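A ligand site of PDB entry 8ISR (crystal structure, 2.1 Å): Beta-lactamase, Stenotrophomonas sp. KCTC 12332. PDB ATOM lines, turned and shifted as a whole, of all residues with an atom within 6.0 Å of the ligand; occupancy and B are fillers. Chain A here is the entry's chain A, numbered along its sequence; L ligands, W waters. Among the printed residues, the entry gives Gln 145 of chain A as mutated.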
ATOM      1  N   MET A  47       5.758  -1.097 -11.417  1.00  0.00           N
ATOM      2  CA  MET A  47       6.507   0.109 -11.746  1.00  0.00           C
ATOM      3  C   MET A  47       7.413   0.547 -10.605  1.00  0.00           C
ATOM      4  O   MET A  47       8.541   1.017 -10.846  1.00  0.00           O
ATOM      5  CB  MET A  47       5.565   1.254 -12.110  1.00  0.00           C
ATOM      6  CG  MET A  47       5.071   1.203 -13.550  1.00  0.00           C
ATOM      7  SD  MET A  47       4.010   2.611 -13.877  1.00  0.00           S
ATOM      8  CE  MET A  47       2.511   2.184 -12.987  1.00  0.00           C
ATOM      9  N   CYS A  48       6.933   0.418  -9.367  1.00  0.00           N
ATOM     10  CA  CYS A  48       7.559   1.076  -8.232  1.00  0.00           C
ATOM     11  C   CYS A  48       7.789   2.541  -8.561  1.00  0.00           C
ATOM     12  O   CYS A  48       6.910   3.198  -9.132  1.00  0.00           O
ATOM     13  CB  CYS A  48       8.880   0.395  -7.839  1.00  0.00           C
ATOM     14  SG  CYS A  48       8.678  -1.345  -7.335  1.00  0.00           S
ATOM     15  N   SER A  49       8.963   3.062  -8.237  1.00  0.00           N
ATOM     16  CA  SER A  49       9.175   4.500  -8.354  1.00  0.00           C
ATOM     17  C   SER A  49       9.286   4.978  -9.801  1.00  0.00           C
ATOM     18  O   SER A  49       9.252   6.197 -10.016  1.00  0.00           O
ATOM     19  CB  SER A  49      10.416   4.930  -7.557  1.00  0.00           C
ATOM     20  OG  SER A  49      10.099   5.033  -6.178  1.00  0.00           O
ATOM     21  N   THR A  50       9.390   4.083 -10.786  1.00  0.00           N
ATOM     22  CA  THR A  50       9.387   4.576 -12.169  1.00  0.00           C
ATOM     23  C   THR A  50       8.048   5.188 -12.563  1.00  0.00           C
ATOM     24  O   THR A  50       7.977   5.832 -13.621  1.00  0.00           O
ATOM     25  CB  THR A  50       9.752   3.482 -13.182  1.00  0.00           C
ATOM     26  OG1 THR A  50       8.707   2.513 -13.249  1.00  0.00           O
ATOM     27  CG2 THR A  50      11.073   2.816 -12.850  1.00  0.00           C
ATOM     28  N   LYS A  52       6.904   7.672 -11.259  1.00  0.00           N
ATOM     29  CA  LYS A  52       7.124   9.104 -11.140  1.00  0.00           C
ATOM     30  C   LYS A  52       7.456   9.749 -12.477  1.00  0.00           C
ATOM     31  O   LYS A  52       7.231  10.951 -12.629  1.00  0.00           O
ATOM     32  CB  LYS A  52       8.227   9.376 -10.110  1.00  0.00           C
ATOM     33  CG  LYS A  52       7.890   8.797  -8.724  1.00  0.00           C
ATOM     34  CD  LYS A  52       9.086   8.892  -7.767  1.00  0.00           C
ATOM     35  CE  LYS A  52       8.787   8.187  -6.445  1.00  0.00           C
ATOM     36  NZ  LYS A  52       9.759   8.484  -5.345  1.00  0.00           N
ATOM     37  N   SER A  83       8.662   7.639   4.473  1.00  0.00           N
ATOM     38  CA  SER A  83      10.075   7.314   4.393  1.00  0.00           C
ATOM     39  C   SER A  83      10.663   7.783   3.073  1.00  0.00           C
ATOM     40  O   SER A  83       9.961   7.874   2.057  1.00  0.00           O
ATOM     41  CB  SER A  83      10.281   5.818   4.555  1.00  0.00           C
ATOM     42  OG  SER A  83       9.834   5.150   3.390  1.00  0.00           O
ATOM     43  N   HIS A  84      11.966   8.078   3.080  1.00  0.00           N
ATOM     44  CA  HIS A  84      12.722   8.369   1.863  1.00  0.00           C
ATOM     45  C   HIS A  84      12.130   9.582   1.116  1.00  0.00           C
ATOM     46  O   HIS A  84      11.792   9.522  -0.077  1.00  0.00           O
ATOM     47  CB  HIS A  84      12.783   7.133   0.974  1.00  0.00           C
ATOM     48  CG  HIS A  84      13.893   7.160  -0.032  1.00  0.00           C
ATOM     49  ND1 HIS A  84      13.862   7.969  -1.149  1.00  0.00           N
ATOM     50  CD2 HIS A  84      15.064   6.482  -0.087  1.00  0.00           C
ATOM     51  CE1 HIS A  84      14.970   7.779  -1.851  1.00  0.00           C
ATOM     52  NE2 HIS A  84      15.710   6.881  -1.232  1.00  0.00           N
ATOM     53  N   ILE A 108      15.896  12.315  -6.807  1.00  0.00           N
ATOM     54  CA  ILE A 108      16.266  11.591  -5.600  1.00  0.00           C
ATOM     55  C   ILE A 108      15.186  10.601  -5.190  1.00  0.00           C
ATOM     56  O   ILE A 108      15.352   9.904  -4.173  1.00  0.00           O
ATOM     57  CB  ILE A 108      16.604  12.564  -4.450  1.00  0.00           C
ATOM     58  CG1 ILE A 108      17.564  11.916  -3.442  1.00  0.00           C
ATOM     59  CG2 ILE A 108      15.357  13.083  -3.732  1.00  0.00           C
ATOM     60  CD1 ILE A 108      18.846  11.380  -4.057  1.00  0.00           C
ATOM     61  N   SER A 109      14.102  10.488  -5.960  1.00  0.00           N
ATOM     62  CA  SER A 109      12.947   9.623  -5.653  1.00  0.00           C
ATOM     63  C   SER A 109      12.347   9.961  -4.298  1.00  0.00           C
ATOM     64  O   SER A 109      12.127   9.097  -3.439  1.00  0.00           O
ATOM     65  CB  SER A 109      13.304   8.135  -5.751  1.00  0.00           C
ATOM     66  OG  SER A 109      12.216   7.399  -6.337  1.00  0.00           O
ATOM     67  N   ASN A 111       9.595  10.334  -1.996  1.00  0.00           N
ATOM     68  CA  ASN A 111       8.318   9.616  -2.037  1.00  0.00           C
ATOM     69  C   ASN A 111       7.151  10.529  -1.692  1.00  0.00           C
ATOM     70  O   ASN A 111       6.096  10.472  -2.340  1.00  0.00           O
ATOM     71  CB  ASN A 111       8.347   8.422  -1.080  1.00  0.00           C
ATOM     72  CG  ASN A 111       9.105   7.240  -1.648  1.00  0.00           C
ATOM     73  OD1 ASN A 111       9.083   7.011  -2.861  1.00  0.00           O
ATOM     74  ND2 ASN A 111       9.761   6.469  -0.785  1.00  0.00           N
ATOM     75  N   GLN A 145       1.996   6.320  -2.924  1.00  0.00           N
ATOM     76  CA  GLN A 145       3.060   5.736  -2.128  1.00  0.00           C
ATOM     77  C   GLN A 145       2.596   5.540  -0.681  1.00  0.00           C
ATOM     78  O   GLN A 145       1.950   6.423  -0.119  1.00  0.00           O
ATOM     79  CB  GLN A 145       4.295   6.641  -2.130  1.00  0.00           C
ATOM     80  CG  GLN A 145       5.027   6.729  -3.483  1.00  0.00           C
ATOM     81  CD  GLN A 145       5.877   5.503  -3.758  1.00  0.00           C
ATOM     82  OE1 GLN A 145       5.446   4.377  -3.552  1.00  0.00           O
ATOM     83  NE2 GLN A 145       7.107   5.723  -4.228  1.00  0.00           N
ATOM     84  N   PRO A 146       2.948   4.406  -0.038  1.00  0.00           N
ATOM     85  CA  PRO A 146       3.801   3.323  -0.551  1.00  0.00           C
ATOM     86  C   PRO A 146       3.068   2.113  -1.122  1.00  0.00           C
ATOM     87  O   PRO A 146       3.731   1.150  -1.508  1.00  0.00           O
ATOM     88  CB  PRO A 146       4.574   2.909   0.697  1.00  0.00           C
ATOM     89  CG  PRO A 146       3.551   3.048   1.797  1.00  0.00           C
ATOM     90  CD  PRO A 146       2.670   4.235   1.400  1.00  0.00           C
ATOM     91  N   ASN A 149       3.735  -0.030  -4.419  1.00  0.00           N
ATOM     92  CA  ASN A 149       4.777  -1.046  -4.489  1.00  0.00           C
ATOM     93  C   ASN A 149       4.232  -2.462  -4.412  1.00  0.00           C
ATOM     94  O   ASN A 149       4.972  -3.403  -4.714  1.00  0.00           O
ATOM     95  CB  ASN A 149       5.816  -0.818  -3.383  1.00  0.00           C
ATOM     96  CG  ASN A 149       6.556   0.505  -3.543  1.00  0.00           C
ATOM     97  OD1 ASN A 149       7.499   0.578  -4.311  1.00  0.00           O
ATOM     98  ND2 ASN A 149       6.129   1.539  -2.810  1.00  0.00           N
ATOM     99  N   THR A 195      20.099   8.760  -8.509  1.00  0.00           N
ATOM    100  CA  THR A 195      19.940   7.418  -7.950  1.00  0.00           C
ATOM    101  C   THR A 195      20.393   6.277  -8.857  1.00  0.00           C
ATOM    102  O   THR A 195      20.234   5.121  -8.479  1.00  0.00           O
ATOM    103  CB  THR A 195      18.468   7.160  -7.594  1.00  0.00           C
ATOM    104  OG1 THR A 195      17.698   7.082  -8.792  1.00  0.00           O
ATOM    105  CG2 THR A 195      17.903   8.273  -6.731  1.00  0.00           C
ATOM    106  N   ARG A 199      23.437   1.477 -11.525  1.00  0.00           N
ATOM    107  CA  ARG A 199      22.432   0.707 -12.262  1.00  0.00           C
ATOM    108  C   ARG A 199      22.768   0.784 -13.756  1.00  0.00           C
ATOM    109  O   ARG A 199      23.899   0.465 -14.121  1.00  0.00           O
ATOM    110  CB  ARG A 199      21.049   1.194 -11.863  1.00  0.00           C
ATOM    111  CG  ARG A 199      20.672   0.749 -10.443  1.00  0.00           C
ATOM    112  CD  ARG A 199      19.809   1.737  -9.707  1.00  0.00           C
ATOM    113  NE  ARG A 199      19.243   1.155  -8.497  1.00  0.00           N
ATOM    114  CZ  ARG A 199      18.510   1.821  -7.586  1.00  0.00           C
ATOM    115  NH1 ARG A 199      18.270   3.128  -7.724  1.00  0.00           N
ATOM    116  NH2 ARG A 199      18.018   1.171  -6.548  1.00  0.00           N
ATOM    117  N   LYS A 213      15.312   7.133 -14.614  1.00  0.00           N
ATOM    118  CA  LYS A 213      14.493   7.115 -13.408  1.00  0.00           C
ATOM    119  C   LYS A 213      14.435   5.688 -12.895  1.00  0.00           C
ATOM    120  O   LYS A 213      14.081   4.770 -13.639  1.00  0.00           O
ATOM    121  CB  LYS A 213      13.073   7.621 -13.653  1.00  0.00           C
ATOM    122  CG  LYS A 213      12.192   7.589 -12.389  1.00  0.00           C
ATOM    123  CD  LYS A 213      12.696   8.602 -11.355  1.00  0.00           C
ATOM    124  CE  LYS A 213      12.074   8.389  -9.960  1.00  0.00           C
ATOM    125  NZ  LYS A 213      12.796   7.354  -9.160  1.00  0.00           N
ATOM    126  N   THR A 214      14.779   5.511 -11.631  1.00  0.00           N
ATOM    127  CA  THR A 214      14.922   4.199 -11.028  1.00  0.00           C
ATOM    128  C   THR A 214      13.714   3.834 -10.161  1.00  0.00           C
ATOM    129  O   THR A 214      12.809   4.637  -9.909  1.00  0.00           O
ATOM    130  CB  THR A 214      16.168   4.180 -10.159  1.00  0.00           C
ATOM    131  OG1 THR A 214      16.052   5.224  -9.188  1.00  0.00           O
ATOM    132  CG2 THR A 214      17.415   4.402 -11.029  1.00  0.00           C
ATOM    133  N   GLY A 215      13.726   2.588  -9.693  1.00  0.00           N
ATOM    134  CA  GLY A 215      12.784   2.137  -8.679  1.00  0.00           C
ATOM    135  C   GLY A 215      13.337   0.942  -7.951  1.00  0.00           C
ATOM    136  O   GLY A 215      14.166   0.201  -8.478  1.00  0.00           O
ATOM    137  N   SER A 216      12.875   0.764  -6.712  1.00  0.00           N
ATOM    138  CA  SER A 216      13.188  -0.442  -5.960  1.00  0.00           C
ATOM    139  C   SER A 216      12.156  -0.600  -4.863  1.00  0.00           C
ATOM    140  O   SER A 216      11.745   0.388  -4.242  1.00  0.00           O
ATOM    141  CB  SER A 216      14.593  -0.403  -5.348  1.00  0.00           C
ATOM    142  OG  SER A 216      14.771  -1.488  -4.443  1.00  0.00           O
ATOM    143  N   ASN A 217      11.763  -1.847  -4.605  1.00  0.00           N
ATOM    144  CA  ASN A 217      10.886  -2.127  -3.468  1.00  0.00           C
ATOM    145  C   ASN A 217      11.668  -2.492  -2.208  1.00  0.00           C
ATOM    146  O   ASN A 217      11.053  -2.853  -1.193  1.00  0.00           O
ATOM    147  CB  ASN A 217       9.859  -3.212  -3.831  1.00  0.00           C
ATOM    148  CG  ASN A 217      10.418  -4.660  -3.774  1.00  0.00           C
ATOM    149  OD1 ASN A 217      11.617  -4.922  -3.788  1.00  0.00           O
ATOM    150  ND2 ASN A 217       9.486  -5.609  -3.714  1.00  0.00           N
ATOM    151  N   GLY A 218      13.002  -2.401  -2.249  1.00  0.00           N
ATOM    152  CA  GLY A 218      13.843  -2.670  -1.101  1.00  0.00           C
ATOM    153  C   GLY A 218      13.978  -4.122  -0.707  1.00  0.00           C
ATOM    154  O   GLY A 218      14.596  -4.426   0.312  1.00  0.00           O
ATOM    155  N   ASN A 223      14.147  -1.436 -10.778  1.00  0.00           N
ATOM    156  CA  ASN A 223      13.837  -0.974 -12.119  1.00  0.00           C
ATOM    157  C   ASN A 223      14.648   0.267 -12.452  1.00  0.00           C
ATOM    158  O   ASN A 223      15.015   1.055 -11.577  1.00  0.00           O
ATOM    159  CB  ASN A 223      12.364  -0.630 -12.302  1.00  0.00           C
ATOM    160  CG  ASN A 223      11.439  -1.677 -11.732  1.00  0.00           C
ATOM    161  OD1 ASN A 223      11.692  -2.874 -11.868  1.00  0.00           O
ATOM    162  ND2 ASN A 223      10.358  -1.230 -11.108  1.00  0.00           N
ATOM    163  N   ASP A 250      19.303  -5.495  -3.089  1.00  0.00           N
ATOM    164  CA  ASP A 250      19.456  -4.301  -3.920  1.00  0.00           C
ATOM    165  C   ASP A 250      20.816  -4.250  -4.598  1.00  0.00           C
ATOM    166  O   ASP A 250      20.909  -3.917  -5.782  1.00  0.00           O
ATOM    167  CB  ASP A 250      19.220  -3.047  -3.074  1.00  0.00           C
ATOM    168  CG  ASP A 250      17.753  -2.665  -3.016  1.00  0.00           C
ATOM    169  OD1 ASP A 250      16.986  -3.354  -2.301  1.00  0.00           O
ATOM    170  OD2 ASP A 250      17.376  -1.699  -3.699  1.00  0.00           O
HETATM  171  C1  LIG L   1      12.335   2.945   1.378  1.00  0.00           C
HETATM  172  C2  LIG L   1      10.749   4.149  -4.209  1.00  0.00           C
HETATM  173  C3  LIG L   1      15.068   4.265  -6.019  1.00  0.00           C
HETATM  174  C4  LIG L   1      11.305   2.718   0.478  1.00  0.00           C
HETATM  175  C5  LIG L   1      11.893   5.156  -4.021  1.00  0.00           C
HETATM  176  C6  LIG L   1      11.413   1.682  -0.448  1.00  0.00           C
HETATM  177  C7  LIG L   1      12.549   0.911  -0.491  1.00  0.00           C
HETATM  178  C8  LIG L   1      13.780   3.692  -2.397  1.00  0.00           C
HETATM  179  C9  LIG L   1      13.576   1.139   0.400  1.00  0.00           C
HETATM  180  C10 LIG L   1      14.624   3.756  -3.638  1.00  0.00           C
HETATM  181  C11 LIG L   1      13.464   2.161   1.326  1.00  0.00           C
HETATM  182  C12 LIG L   1      14.146   4.142  -4.814  1.00  0.00           C
HETATM  183  C13 LIG L   1      10.283   1.446  -1.446  1.00  0.00           C
HETATM  184  C14 LIG L   1      10.136   2.720  -2.280  1.00  0.00           C
HETATM  185  C15 LIG L   1      10.630   3.856  -5.713  1.00  0.00           C
HETATM  186  N1  LIG L   1       9.044   1.151  -0.741  1.00  0.00           N
HETATM  187  N2  LIG L   1      10.935   2.912  -3.476  1.00  0.00           N
HETATM  188  N3  LIG L   1      12.926   4.917  -5.029  1.00  0.00           N
HETATM  189  O1  LIG L   1       9.378   3.578  -1.970  1.00  0.00           O
HETATM  190  O2  LIG L   1      10.873   2.791  -6.169  1.00  0.00           O
HETATM  191  O3  LIG L   1      16.279   3.970  -5.967  1.00  0.00           O
HETATM  192  O4  LIG L   1      14.564   4.715  -7.088  1.00  0.00           O
HETATM  193  S1  LIG L   1      12.698   5.115  -2.404  1.00  0.00           S
HETATM  194 CL1  LIG L   1      16.095   2.741  -3.546  1.00  0.00          CL
HETATM  195  O   HOH W   1       7.029   4.731  -0.575  1.00  0.00           O
HETATM  196  O   HOH W   2       7.841   3.071  -5.266  1.00  0.00           O
HETATM  197  O   HOH W   3      18.470   0.608  -3.192  1.00  0.00           O
HETATM  198  O   HOH W   4       8.121  -2.179  -0.898  1.00  0.00           O
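Water W1 lies within hydrogen-bond range of an oxygen (O1) of the ligand (3.0 Å), the side-chain amide nitrogen (ND2) of Asn 111 (3.2 Å) and the side-chain amide oxygen (OE1) of Gln 145 (3.4 Å).
Water W3 lies within hydrogen-bond range of OD2 of Asp 250 and NH2 of Arg 199.
Water W4 bridges the backbone carbonyl oxygen (O) of Asn 217 (3.0 Å) and a nitrogen (N1) of the ligand (3.5 Å).
The side-chain amide oxygen of Asn 111 is in hydrogen-bond range of the side-chain amino group of Lys 52 (3.0 Å).
OG of Ser 216 sits at hydrogen-bond distance from N of Gly 218 (3.0 Å).
The backbone NH of Gly 215 sits at hydrogen-bond distance from the backbone carbonyl oxygen of Asn 223, 2.7 Å away.
The side-chain amide nitrogen (ND2) of Asn 111 is in hydrogen-bond range of the backbone carbonyl oxygen (O) of Ser 83.
The backbone NH of Asn 111 lies within hydrogen-bond range of the backbone carbonyl oxygen of His 84 (3.0 Å).
The side-chain amide oxygen of Asn 149 lies within hydrogen-bond range of the side-chain sulfur of Cys 48, 3.8 Å away.
ND2 of Asn 149 lies within hydrogen-bond range of OE1 of Gln 145.
OG of Ser 109 is in hydrogen-bond range of NZ of Lys 52 (2.9 Å).
Merely in contact with the ligand: Cys 48, Asn 149, Gly 218, Gln 145, Ser 83 and Asn 217.
Hydrophobic or aromatic side chains within 4 Å of the ligand: His 84.
Within 4 Å of the ligand: Cys 48, Ser 49, Ser 83, His 84, Ser 109, Asn 111, Gln 145, Asn 149, Arg 199, Lys 213, Thr 214, Gly 215, Ser 216, Asn 217 and Gly 218.
The nearest printed residue that does not touch the ligand is Lys 52 (4.2 Å).
NH1 of Arg 199 is in salt-bridge range of O3 of the ligand, 2.8 Å away.
ND2 of Asn 111 sits at hydrogen-bond distance from O1 of the ligand (3.1 Å).
NZ of Lys 213 lies within salt-bridge range of O4 of the ligand (3.8 Å).
OG1 of Thr 214 is in hydrogen-bond range of O4 of the ligand.
A ring nitrogen (ND1) of His 84 sits close to a sulfur (S1) of the ligand (3.3 Å).
OG of Ser 49 is covalently linked to C15 of the ligand (1.4 Å).
The backbone NH of Ser 49 lies close to an oxygen (O2) of the ligand, 2.8 Å away.
O2 of the ligand lies within hydrogen-bond range of N of Ser 216.
N of Gly 215 lies within hydrogen-bond range of O4 of the ligand, at 3.5 Å.
OG of Ser 109 lies within hydrogen-bond range of N3 of the ligand (2.9 Å).
The backbone carbonyl oxygen (O) of Ser 216 is in hydrogen-bond range of a nitrogen (N2) of the ligand (2.8 Å).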
